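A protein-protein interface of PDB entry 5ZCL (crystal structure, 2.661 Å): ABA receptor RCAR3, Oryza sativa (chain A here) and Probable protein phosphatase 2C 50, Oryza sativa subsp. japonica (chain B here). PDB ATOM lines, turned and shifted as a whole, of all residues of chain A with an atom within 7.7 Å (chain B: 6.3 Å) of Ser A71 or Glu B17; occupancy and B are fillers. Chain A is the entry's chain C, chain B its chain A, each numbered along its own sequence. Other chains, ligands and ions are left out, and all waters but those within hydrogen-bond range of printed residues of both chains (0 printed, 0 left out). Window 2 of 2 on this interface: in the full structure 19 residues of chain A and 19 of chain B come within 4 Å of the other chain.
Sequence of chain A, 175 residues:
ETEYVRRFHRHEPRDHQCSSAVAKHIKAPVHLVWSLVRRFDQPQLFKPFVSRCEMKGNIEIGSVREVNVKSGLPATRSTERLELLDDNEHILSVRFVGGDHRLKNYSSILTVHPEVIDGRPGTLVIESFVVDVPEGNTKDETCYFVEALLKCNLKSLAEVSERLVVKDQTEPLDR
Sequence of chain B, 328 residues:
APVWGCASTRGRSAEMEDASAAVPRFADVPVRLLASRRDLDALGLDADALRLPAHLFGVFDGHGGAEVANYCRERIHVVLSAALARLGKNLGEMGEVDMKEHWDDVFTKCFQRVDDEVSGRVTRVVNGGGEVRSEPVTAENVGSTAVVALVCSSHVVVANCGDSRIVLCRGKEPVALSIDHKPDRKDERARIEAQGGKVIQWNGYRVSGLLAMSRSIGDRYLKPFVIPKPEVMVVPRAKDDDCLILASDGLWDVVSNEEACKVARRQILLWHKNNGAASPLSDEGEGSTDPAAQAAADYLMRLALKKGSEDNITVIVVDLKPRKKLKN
O of Glu B17 is in hydrogen-bond range of N of Gly B62, 2.9 Å away. OE2 of Glu B17 is in hydrogen-bond range of N of Gly B65, 3.2 Å away. OD1 of Asn B312 is in hydrogen-bond range of N of Glu B17, at 2.8 Å. The backbone NH (N) of Lys A70 is in hydrogen-bond range of the backbone carbonyl oxygen (O) of Phe A49 (2.8 Å).
Of the 11 printed residues of chain A, 4 touch a printed residue of chain B. Printed residues of chain A that touch a printed residue of chain B: Phe A49, Lys A70, Ser A71 and Gly A72. Hydrophobic or aromatic side chains of chain B within 4 Å of the printed part of chain A: His B63. Among the printed residues, 6 pairs touch across the chains.
The side-chain hydroxyl (OG) of Ser A71 sits at hydrogen-bond distance from the side-chain carboxylate (OE1) of Glu B17 (2.6 Å). The side-chain hydroxyl (OG) of Ser A71 is in hydrogen-bond range of the backbone NH (N) of Gly B64, at 2.8 Å.
Glu B17 touches just one residue of chain A: Ser A71. Of the printed residues of chain B, Phe A49 touches Asn B141. Printed residues of chain A within 4 Å of His B63: Ser A71 and Gly A72. Printed residues of chain A within 4 Å of Asn B141: Phe A49. Of the printed residues of chain B, Gly A72 touches His B63. Asn B70 touches none of the printed residues of chain A. Ala B19 touches none of the printed residues of chain A. The nearest printed residue of chain A that does not touch Glu B17 is Gly A72 (5.9 Å).
ND2 of Asn B141 touches CD1 of Phe A49, 3.5 Å away. Lys A70 touches Gly B64 (CD to O, 3.7 Å). OG of Ser A71 touches CA of His B63 (3.5 Å). CB of His B63 touches CA of Gly A72, 3.9 Å away.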
ATOM      1  N   PHE A  49      27.020  25.980   8.906  1.00  0.00           N
ATOM      2  CA  PHE A  49      28.139  26.360   8.061  1.00  0.00           C
ATOM      3  C   PHE A  49      29.199  25.278   7.944  1.00  0.00           C
ATOM      4  O   PHE A  49      30.105  25.410   7.111  1.00  0.00           O
ATOM      5  CB  PHE A  49      28.783  27.632   8.607  1.00  0.00           C
ATOM      6  CG  PHE A  49      27.937  28.849   8.435  1.00  0.00           C
ATOM      7  CD1 PHE A  49      27.830  29.457   7.198  1.00  0.00           C
ATOM      8  CD2 PHE A  49      27.254  29.391   9.514  1.00  0.00           C
ATOM      9  CE1 PHE A  49      27.044  30.576   7.030  1.00  0.00           C
ATOM     10  CE2 PHE A  49      26.470  30.512   9.356  1.00  0.00           C
ATOM     11  CZ  PHE A  49      26.365  31.108   8.110  1.00  0.00           C
ATOM     12  N   SER A  51      30.594  21.708   6.823  1.00  0.00           N
ATOM     13  CA  SER A  51      30.356  20.637   5.867  1.00  0.00           C
ATOM     14  C   SER A  51      31.043  19.342   6.241  1.00  0.00           C
ATOM     15  O   SER A  51      30.540  18.271   5.908  1.00  0.00           O
ATOM     16  CB  SER A  51      30.820  21.041   4.464  1.00  0.00           C
ATOM     17  OG  SER A  51      32.221  21.172   4.421  1.00  0.00           O
ATOM     18  N   ASN A  68      35.829  21.904   8.154  1.00  0.00           N
ATOM     19  CA  ASN A  68      35.750  22.496   6.822  1.00  0.00           C
ATOM     20  C   ASN A  68      34.382  23.132   6.658  1.00  0.00           C
ATOM     21  O   ASN A  68      33.360  22.474   6.887  1.00  0.00           O
ATOM     22  CB  ASN A  68      35.987  21.462   5.719  1.00  0.00           C
ATOM     23  CG  ASN A  68      37.459  21.196   5.486  1.00  0.00           C
ATOM     24  OD1 ASN A  68      38.157  22.011   4.888  1.00  0.00           O
ATOM     25  ND2 ASN A  68      37.940  20.056   5.958  1.00  0.00           N
ATOM     26  N   VAL A  69      34.359  24.396   6.251  1.00  0.00           N
ATOM     27  CA  VAL A  69      33.116  25.140   6.171  1.00  0.00           C
ATOM     28  C   VAL A  69      32.635  25.150   4.729  1.00  0.00           C
ATOM     29  O   VAL A  69      33.393  24.901   3.787  1.00  0.00           O
ATOM     30  CB  VAL A  69      33.257  26.574   6.717  1.00  0.00           C
ATOM     31  CG1 VAL A  69      33.522  26.539   8.215  1.00  0.00           C
ATOM     32  CG2 VAL A  69      34.362  27.292   5.984  1.00  0.00           C
ATOM     33  N   LYS A  70      31.346  25.448   4.559  1.00  0.00           N
ATOM     34  CA  LYS A  70      30.702  25.455   3.261  1.00  0.00           C
ATOM     35  C   LYS A  70      31.116  26.692   2.468  1.00  0.00           C
ATOM     36  O   LYS A  70      31.733  27.619   2.988  1.00  0.00           O
ATOM     37  CB  LYS A  70      29.181  25.398   3.429  1.00  0.00           C
ATOM     38  CG  LYS A  70      28.704  24.286   4.348  1.00  0.00           C
ATOM     39  CD  LYS A  70      27.232  23.964   4.134  1.00  0.00           C
ATOM     40  CE  LYS A  70      26.775  22.805   5.014  1.00  0.00           C
ATOM     41  NZ  LYS A  70      25.398  23.006   5.524  1.00  0.00           N
ATOM     42  N   SER A  71      30.743  26.707   1.190  1.00  0.00           N
ATOM     43  CA  SER A  71      31.093  27.801   0.296  1.00  0.00           C
ATOM     44  C   SER A  71      30.302  29.061   0.660  1.00  0.00           C
ATOM     45  O   SER A  71      29.366  29.039   1.469  1.00  0.00           O
ATOM     46  CB  SER A  71      30.820  27.413  -1.149  1.00  0.00           C
ATOM     47  OG  SER A  71      29.447  27.085  -1.317  1.00  0.00           O
ATOM     48  N   GLY A  72      30.714  30.186   0.075  1.00  0.00           N
ATOM     49  CA  GLY A  72      30.068  31.451   0.373  1.00  0.00           C
ATOM     50  C   GLY A  72      30.504  32.121   1.657  1.00  0.00           C
ATOM     51  O   GLY A  72      29.737  32.906   2.223  1.00  0.00           O
ATOM     52  N   LEU A  73      31.701  31.824   2.144  1.00  0.00           N
ATOM     53  CA  LEU A  73      32.254  32.389   3.369  1.00  0.00           C
ATOM     54  C   LEU A  73      33.639  32.927   3.076  1.00  0.00           C
ATOM     55  O   LEU A  73      34.236  32.628   2.038  1.00  0.00           O
ATOM     56  CB  LEU A  73      32.328  31.344   4.494  1.00  0.00           C
ATOM     57  CG  LEU A  73      31.044  30.791   5.116  1.00  0.00           C
ATOM     58  CD1 LEU A  73      31.374  29.544   5.904  1.00  0.00           C
ATOM     59  CD2 LEU A  73      30.406  31.817   6.024  1.00  0.00           C
ATOM     60  N   PRO A  74      34.185  33.739   3.980  1.00  0.00           N
ATOM     61  CA  PRO A  74      35.543  34.262   3.798  1.00  0.00           C
ATOM     62  C   PRO A  74      36.643  33.258   4.116  1.00  0.00           C
ATOM     63  O   PRO A  74      37.822  33.599   3.973  1.00  0.00           O
ATOM     64  CB  PRO A  74      35.590  35.449   4.778  1.00  0.00           C
ATOM     65  CG  PRO A  74      34.182  35.674   5.217  1.00  0.00           C
ATOM     66  CD  PRO A  74      33.498  34.355   5.119  1.00  0.00           C
ATOM     67  N   ALA A  75      36.317  32.057   4.586  1.00  0.00           N
ATOM     68  CA  ALA A  75      37.329  31.077   4.949  1.00  0.00           C
ATOM     69  C   ALA A  75      36.829  29.688   4.577  1.00  0.00           C
ATOM     70  O   ALA A  75      35.657  29.500   4.254  1.00  0.00           O
ATOM     71  CB  ALA A  75      37.668  31.163   6.449  1.00  0.00           C
ATOM     72  N   THR A  76      37.722  28.701   4.644  1.00  0.00           N
ATOM     73  CA  THR A  76      37.372  27.328   4.307  1.00  0.00           C
ATOM     74  C   THR A  76      37.618  26.324   5.419  1.00  0.00           C
ATOM     75  O   THR A  76      36.926  25.305   5.465  1.00  0.00           O
ATOM     76  CB  THR A  76      38.155  26.845   3.070  1.00  0.00           C
ATOM     77  OG1 THR A  76      39.546  26.705   3.391  1.00  0.00           O
ATOM     78  CG2 THR A  76      38.008  27.809   1.935  1.00  0.00           C
ATOM     79  N   GLU B  15      32.877  20.044  -5.146  1.00  0.00           N
ATOM     80  CA  GLU B  15      31.464  19.858  -5.430  1.00  0.00           C
ATOM     81  C   GLU B  15      31.012  20.811  -6.527  1.00  0.00           C
ATOM     82  O   GLU B  15      31.660  21.817  -6.818  1.00  0.00           O
ATOM     83  CB  GLU B  15      30.618  20.099  -4.172  1.00  0.00           C
ATOM     84  CG  GLU B  15      30.699  19.010  -3.118  1.00  0.00           C
ATOM     85  CD  GLU B  15      30.325  19.533  -1.738  1.00  0.00           C
ATOM     86  OE1 GLU B  15      31.242  19.743  -0.913  1.00  0.00           O
ATOM     87  OE2 GLU B  15      29.118  19.761  -1.487  1.00  0.00           O
ATOM     88  N   MET B  16      29.891  20.465  -7.151  1.00  0.00           N
ATOM     89  CA  MET B  16      29.270  21.292  -8.174  1.00  0.00           C
ATOM     90  C   MET B  16      28.108  22.037  -7.535  1.00  0.00           C
ATOM     91  O   MET B  16      27.197  21.410  -6.986  1.00  0.00           O
ATOM     92  CB  MET B  16      28.789  20.449  -9.353  1.00  0.00           C
ATOM     93  CG  MET B  16      28.143  21.254 -10.478  1.00  0.00           C
ATOM     94  SD  MET B  16      29.209  22.595 -11.034  1.00  0.00           S
ATOM     95  CE  MET B  16      28.718  22.781 -12.745  1.00  0.00           C
ATOM     96  N   GLU B  17      28.155  23.370  -7.578  1.00  0.00           N
ATOM     97  CA  GLU B  17      27.059  24.182  -7.072  1.00  0.00           C
ATOM     98  C   GLU B  17      26.521  25.164  -8.099  1.00  0.00           C
ATOM     99  O   GLU B  17      25.583  25.904  -7.792  1.00  0.00           O
ATOM    100  CB  GLU B  17      27.488  24.936  -5.807  1.00  0.00           C
ATOM    101  CG  GLU B  17      27.823  24.012  -4.660  1.00  0.00           C
ATOM    102  CD  GLU B  17      28.325  24.737  -3.427  1.00  0.00           C
ATOM    103  OE1 GLU B  17      28.768  25.905  -3.552  1.00  0.00           O
ATOM    104  OE2 GLU B  17      28.261  24.130  -2.330  1.00  0.00           O
ATOM    105  N   ASP B  18      27.083  25.188  -9.303  1.00  0.00           N
ATOM    106  CA  ASP B  18      26.511  25.914 -10.426  1.00  0.00           C
ATOM    107  C   ASP B  18      25.337  25.134 -11.005  1.00  0.00           C
ATOM    108  O   ASP B  18      25.290  23.903 -10.950  1.00  0.00           O
ATOM    109  CB  ASP B  18      27.568  26.135 -11.517  1.00  0.00           C
ATOM    110  CG  ASP B  18      28.378  27.425 -11.326  1.00  0.00           C
ATOM    111  OD1 ASP B  18      28.293  28.063 -10.255  1.00  0.00           O
ATOM    112  OD2 ASP B  18      29.116  27.794 -12.261  1.00  0.00           O
ATOM    113  N   ALA B  19      24.374  25.867 -11.555  1.00  0.00           N
ATOM    114  CA  ALA B  19      23.272  25.286 -12.309  1.00  0.00           C
ATOM    115  C   ALA B  19      22.984  26.187 -13.500  1.00  0.00           C
ATOM    116  O   ALA B  19      23.399  27.346 -13.532  1.00  0.00           O
ATOM    117  CB  ALA B  19      22.013  25.104 -11.448  1.00  0.00           C
ATOM    118  N   PHE B  60      23.040  30.076 -12.558  1.00  0.00           N
ATOM    119  CA  PHE B  60      22.804  30.215 -11.126  1.00  0.00           C
ATOM    120  C   PHE B  60      24.015  29.666 -10.388  1.00  0.00           C
ATOM    121  O   PHE B  60      24.218  28.450 -10.329  1.00  0.00           O
ATOM    122  CB  PHE B  60      21.520  29.500 -10.730  1.00  0.00           C
ATOM    123  CG  PHE B  60      20.420  29.683 -11.725  1.00  0.00           C
ATOM    124  CD1 PHE B  60      19.608  30.799 -11.683  1.00  0.00           C
ATOM    125  CD2 PHE B  60      20.202  28.745 -12.715  1.00  0.00           C
ATOM    126  CE1 PHE B  60      18.594  30.971 -12.620  1.00  0.00           C
ATOM    127  CE2 PHE B  60      19.187  28.911 -13.646  1.00  0.00           C
ATOM    128  CZ  PHE B  60      18.383  30.024 -13.594  1.00  0.00           C
ATOM    129  N   ASP B  61      24.841  30.561  -9.860  1.00  0.00           N
ATOM    130  CA  ASP B  61      25.993  30.169  -9.059  1.00  0.00           C
ATOM    131  C   ASP B  61      25.516  29.991  -7.630  1.00  0.00           C
ATOM    132  O   ASP B  61      25.204  30.972  -6.951  1.00  0.00           O
ATOM    133  CB  ASP B  61      27.105  31.211  -9.129  1.00  0.00           C
ATOM    134  CG  ASP B  61      28.360  30.774  -8.396  1.00  0.00           C
ATOM    135  OD1 ASP B  61      28.251  29.914  -7.480  1.00  0.00           O
ATOM    136  OD2 ASP B  61      29.452  31.298  -8.739  1.00  0.00           O
ATOM    137  N   GLY B  62      25.451  28.743  -7.177  1.00  0.00           N
ATOM    138  CA  GLY B  62      25.089  28.484  -5.803  1.00  0.00           C
ATOM    139  C   GLY B  62      26.248  28.707  -4.847  1.00  0.00           C
ATOM    140  O   GLY B  62      27.426  28.600  -5.202  1.00  0.00           O
ATOM    141  N   HIS B  63      25.890  29.056  -3.616  1.00  0.00           N
ATOM    142  CA  HIS B  63      26.828  29.107  -2.508  1.00  0.00           C
ATOM    143  C   HIS B  63      26.156  28.492  -1.293  1.00  0.00           C
ATOM    144  O   HIS B  63      24.925  28.526  -1.164  1.00  0.00           O
ATOM    145  CB  HIS B  63      27.286  30.537  -2.198  1.00  0.00           C
ATOM    146  CG  HIS B  63      26.165  31.519  -2.100  1.00  0.00           C
ATOM    147  ND1 HIS B  63      25.877  32.420  -3.104  1.00  0.00           N
ATOM    148  CD2 HIS B  63      25.264  31.749  -1.116  1.00  0.00           C
ATOM    149  CE1 HIS B  63      24.839  33.155  -2.746  1.00  0.00           C
ATOM    150  NE2 HIS B  63      24.455  32.775  -1.539  1.00  0.00           N
ATOM    151  N   GLY B  64      26.975  27.923  -0.406  1.00  0.00           N
ATOM    152  CA  GLY B  64      26.463  27.209   0.746  1.00  0.00           C
ATOM    153  C   GLY B  64      25.769  25.909   0.416  1.00  0.00           C
ATOM    154  O   GLY B  64      25.233  25.262   1.323  1.00  0.00           O
ATOM    155  N   GLY B  65      25.775  25.507  -0.842  1.00  0.00           N
ATOM    156  CA  GLY B  65      25.050  24.337  -1.295  1.00  0.00           C
ATOM    157  C   GLY B  65      24.570  24.536  -2.716  1.00  0.00           C
ATOM    158  O   GLY B  65      24.600  25.637  -3.266  1.00  0.00           O
ATOM    159  N   ALA B  66      24.121  23.439  -3.313  1.00  0.00           N
ATOM    160  CA  ALA B  66      23.638  23.485  -4.678  1.00  0.00           C
ATOM    161  C   ALA B  66      22.122  23.568  -4.763  1.00  0.00           C
ATOM    162  O   ALA B  66      21.591  23.804  -5.855  1.00  0.00           O
ATOM    163  CB  ALA B  66      24.128  22.258  -5.462  1.00  0.00           C
ATOM    164  N   ALA B  69      20.556  26.939  -6.227  1.00  0.00           N
ATOM    165  CA  ALA B  69      20.862  27.060  -7.648  1.00  0.00           C
ATOM    166  C   ALA B  69      20.059  26.051  -8.463  1.00  0.00           C
ATOM    167  O   ALA B  69      19.465  26.398  -9.487  1.00  0.00           O
ATOM    168  CB  ALA B  69      22.357  26.879  -7.886  1.00  0.00           C
ATOM    169  N   ASN B  70      20.011  24.794  -8.008  1.00  0.00           N
ATOM    170  CA  ASN B  70      19.203  23.792  -8.700  1.00  0.00           C
ATOM    171  C   ASN B  70      17.730  24.182  -8.713  1.00  0.00           C
ATOM    172  O   ASN B  70      17.038  24.009  -9.724  1.00  0.00           O
ATOM    173  CB  ASN B  70      19.367  22.418  -8.047  1.00  0.00           C
ATOM    174  CG  ASN B  70      20.750  21.845  -8.231  1.00  0.00           C
ATOM    175  OD1 ASN B  70      21.458  22.189  -9.178  1.00  0.00           O
ATOM    176  ND2 ASN B  70      21.138  20.939  -7.339  1.00  0.00           N
ATOM    177  N   ASN B 141      21.310  29.414   5.172  1.00  0.00           N
ATOM    178  CA  ASN B 141      22.600  29.920   4.710  1.00  0.00           C
ATOM    179  C   ASN B 141      22.941  29.470   3.289  1.00  0.00           C
ATOM    180  O   ASN B 141      24.103  29.550   2.878  1.00  0.00           O
ATOM    181  CB  ASN B 141      23.716  29.496   5.659  1.00  0.00           C
ATOM    182  CG  ASN B 141      24.030  28.011   5.572  1.00  0.00           C
ATOM    183  OD1 ASN B 141      23.135  27.171   5.443  1.00  0.00           O
ATOM    184  ND2 ASN B 141      25.311  27.681   5.641  1.00  0.00           N
ATOM    185  N   SER B 144      21.922  31.588  -4.082  1.00  0.00           N
ATOM    186  CA  SER B 144      22.385  31.444  -5.451  1.00  0.00           C
ATOM    187  C   SER B 144      22.206  32.763  -6.183  1.00  0.00           C
ATOM    188  O   SER B 144      21.218  33.468  -5.965  1.00  0.00           O
ATOM    189  CB  SER B 144      21.615  30.330  -6.168  1.00  0.00           C
ATOM    190  OG  SER B 144      21.968  30.277  -7.539  1.00  0.00           O
ATOM    191  N   ASN B 312      33.701  26.584  -9.576  1.00  0.00           N
ATOM    192  CA  ASN B 312      32.816  26.047 -10.606  1.00  0.00           C
ATOM    193  C   ASN B 312      32.758  27.016 -11.781  1.00  0.00           C
ATOM    194  O   ASN B 312      32.902  28.232 -11.613  1.00  0.00           O
ATOM    195  CB  ASN B 312      31.394  25.819 -10.079  1.00  0.00           C
ATOM    196  CG  ASN B 312      31.337  24.881  -8.887  1.00  0.00           C
ATOM    197  OD1 ASN B 312      30.433  24.984  -8.056  1.00  0.00           O
ATOM    198  ND2 ASN B 312      32.298  23.968  -8.794  1.00  0.00           N
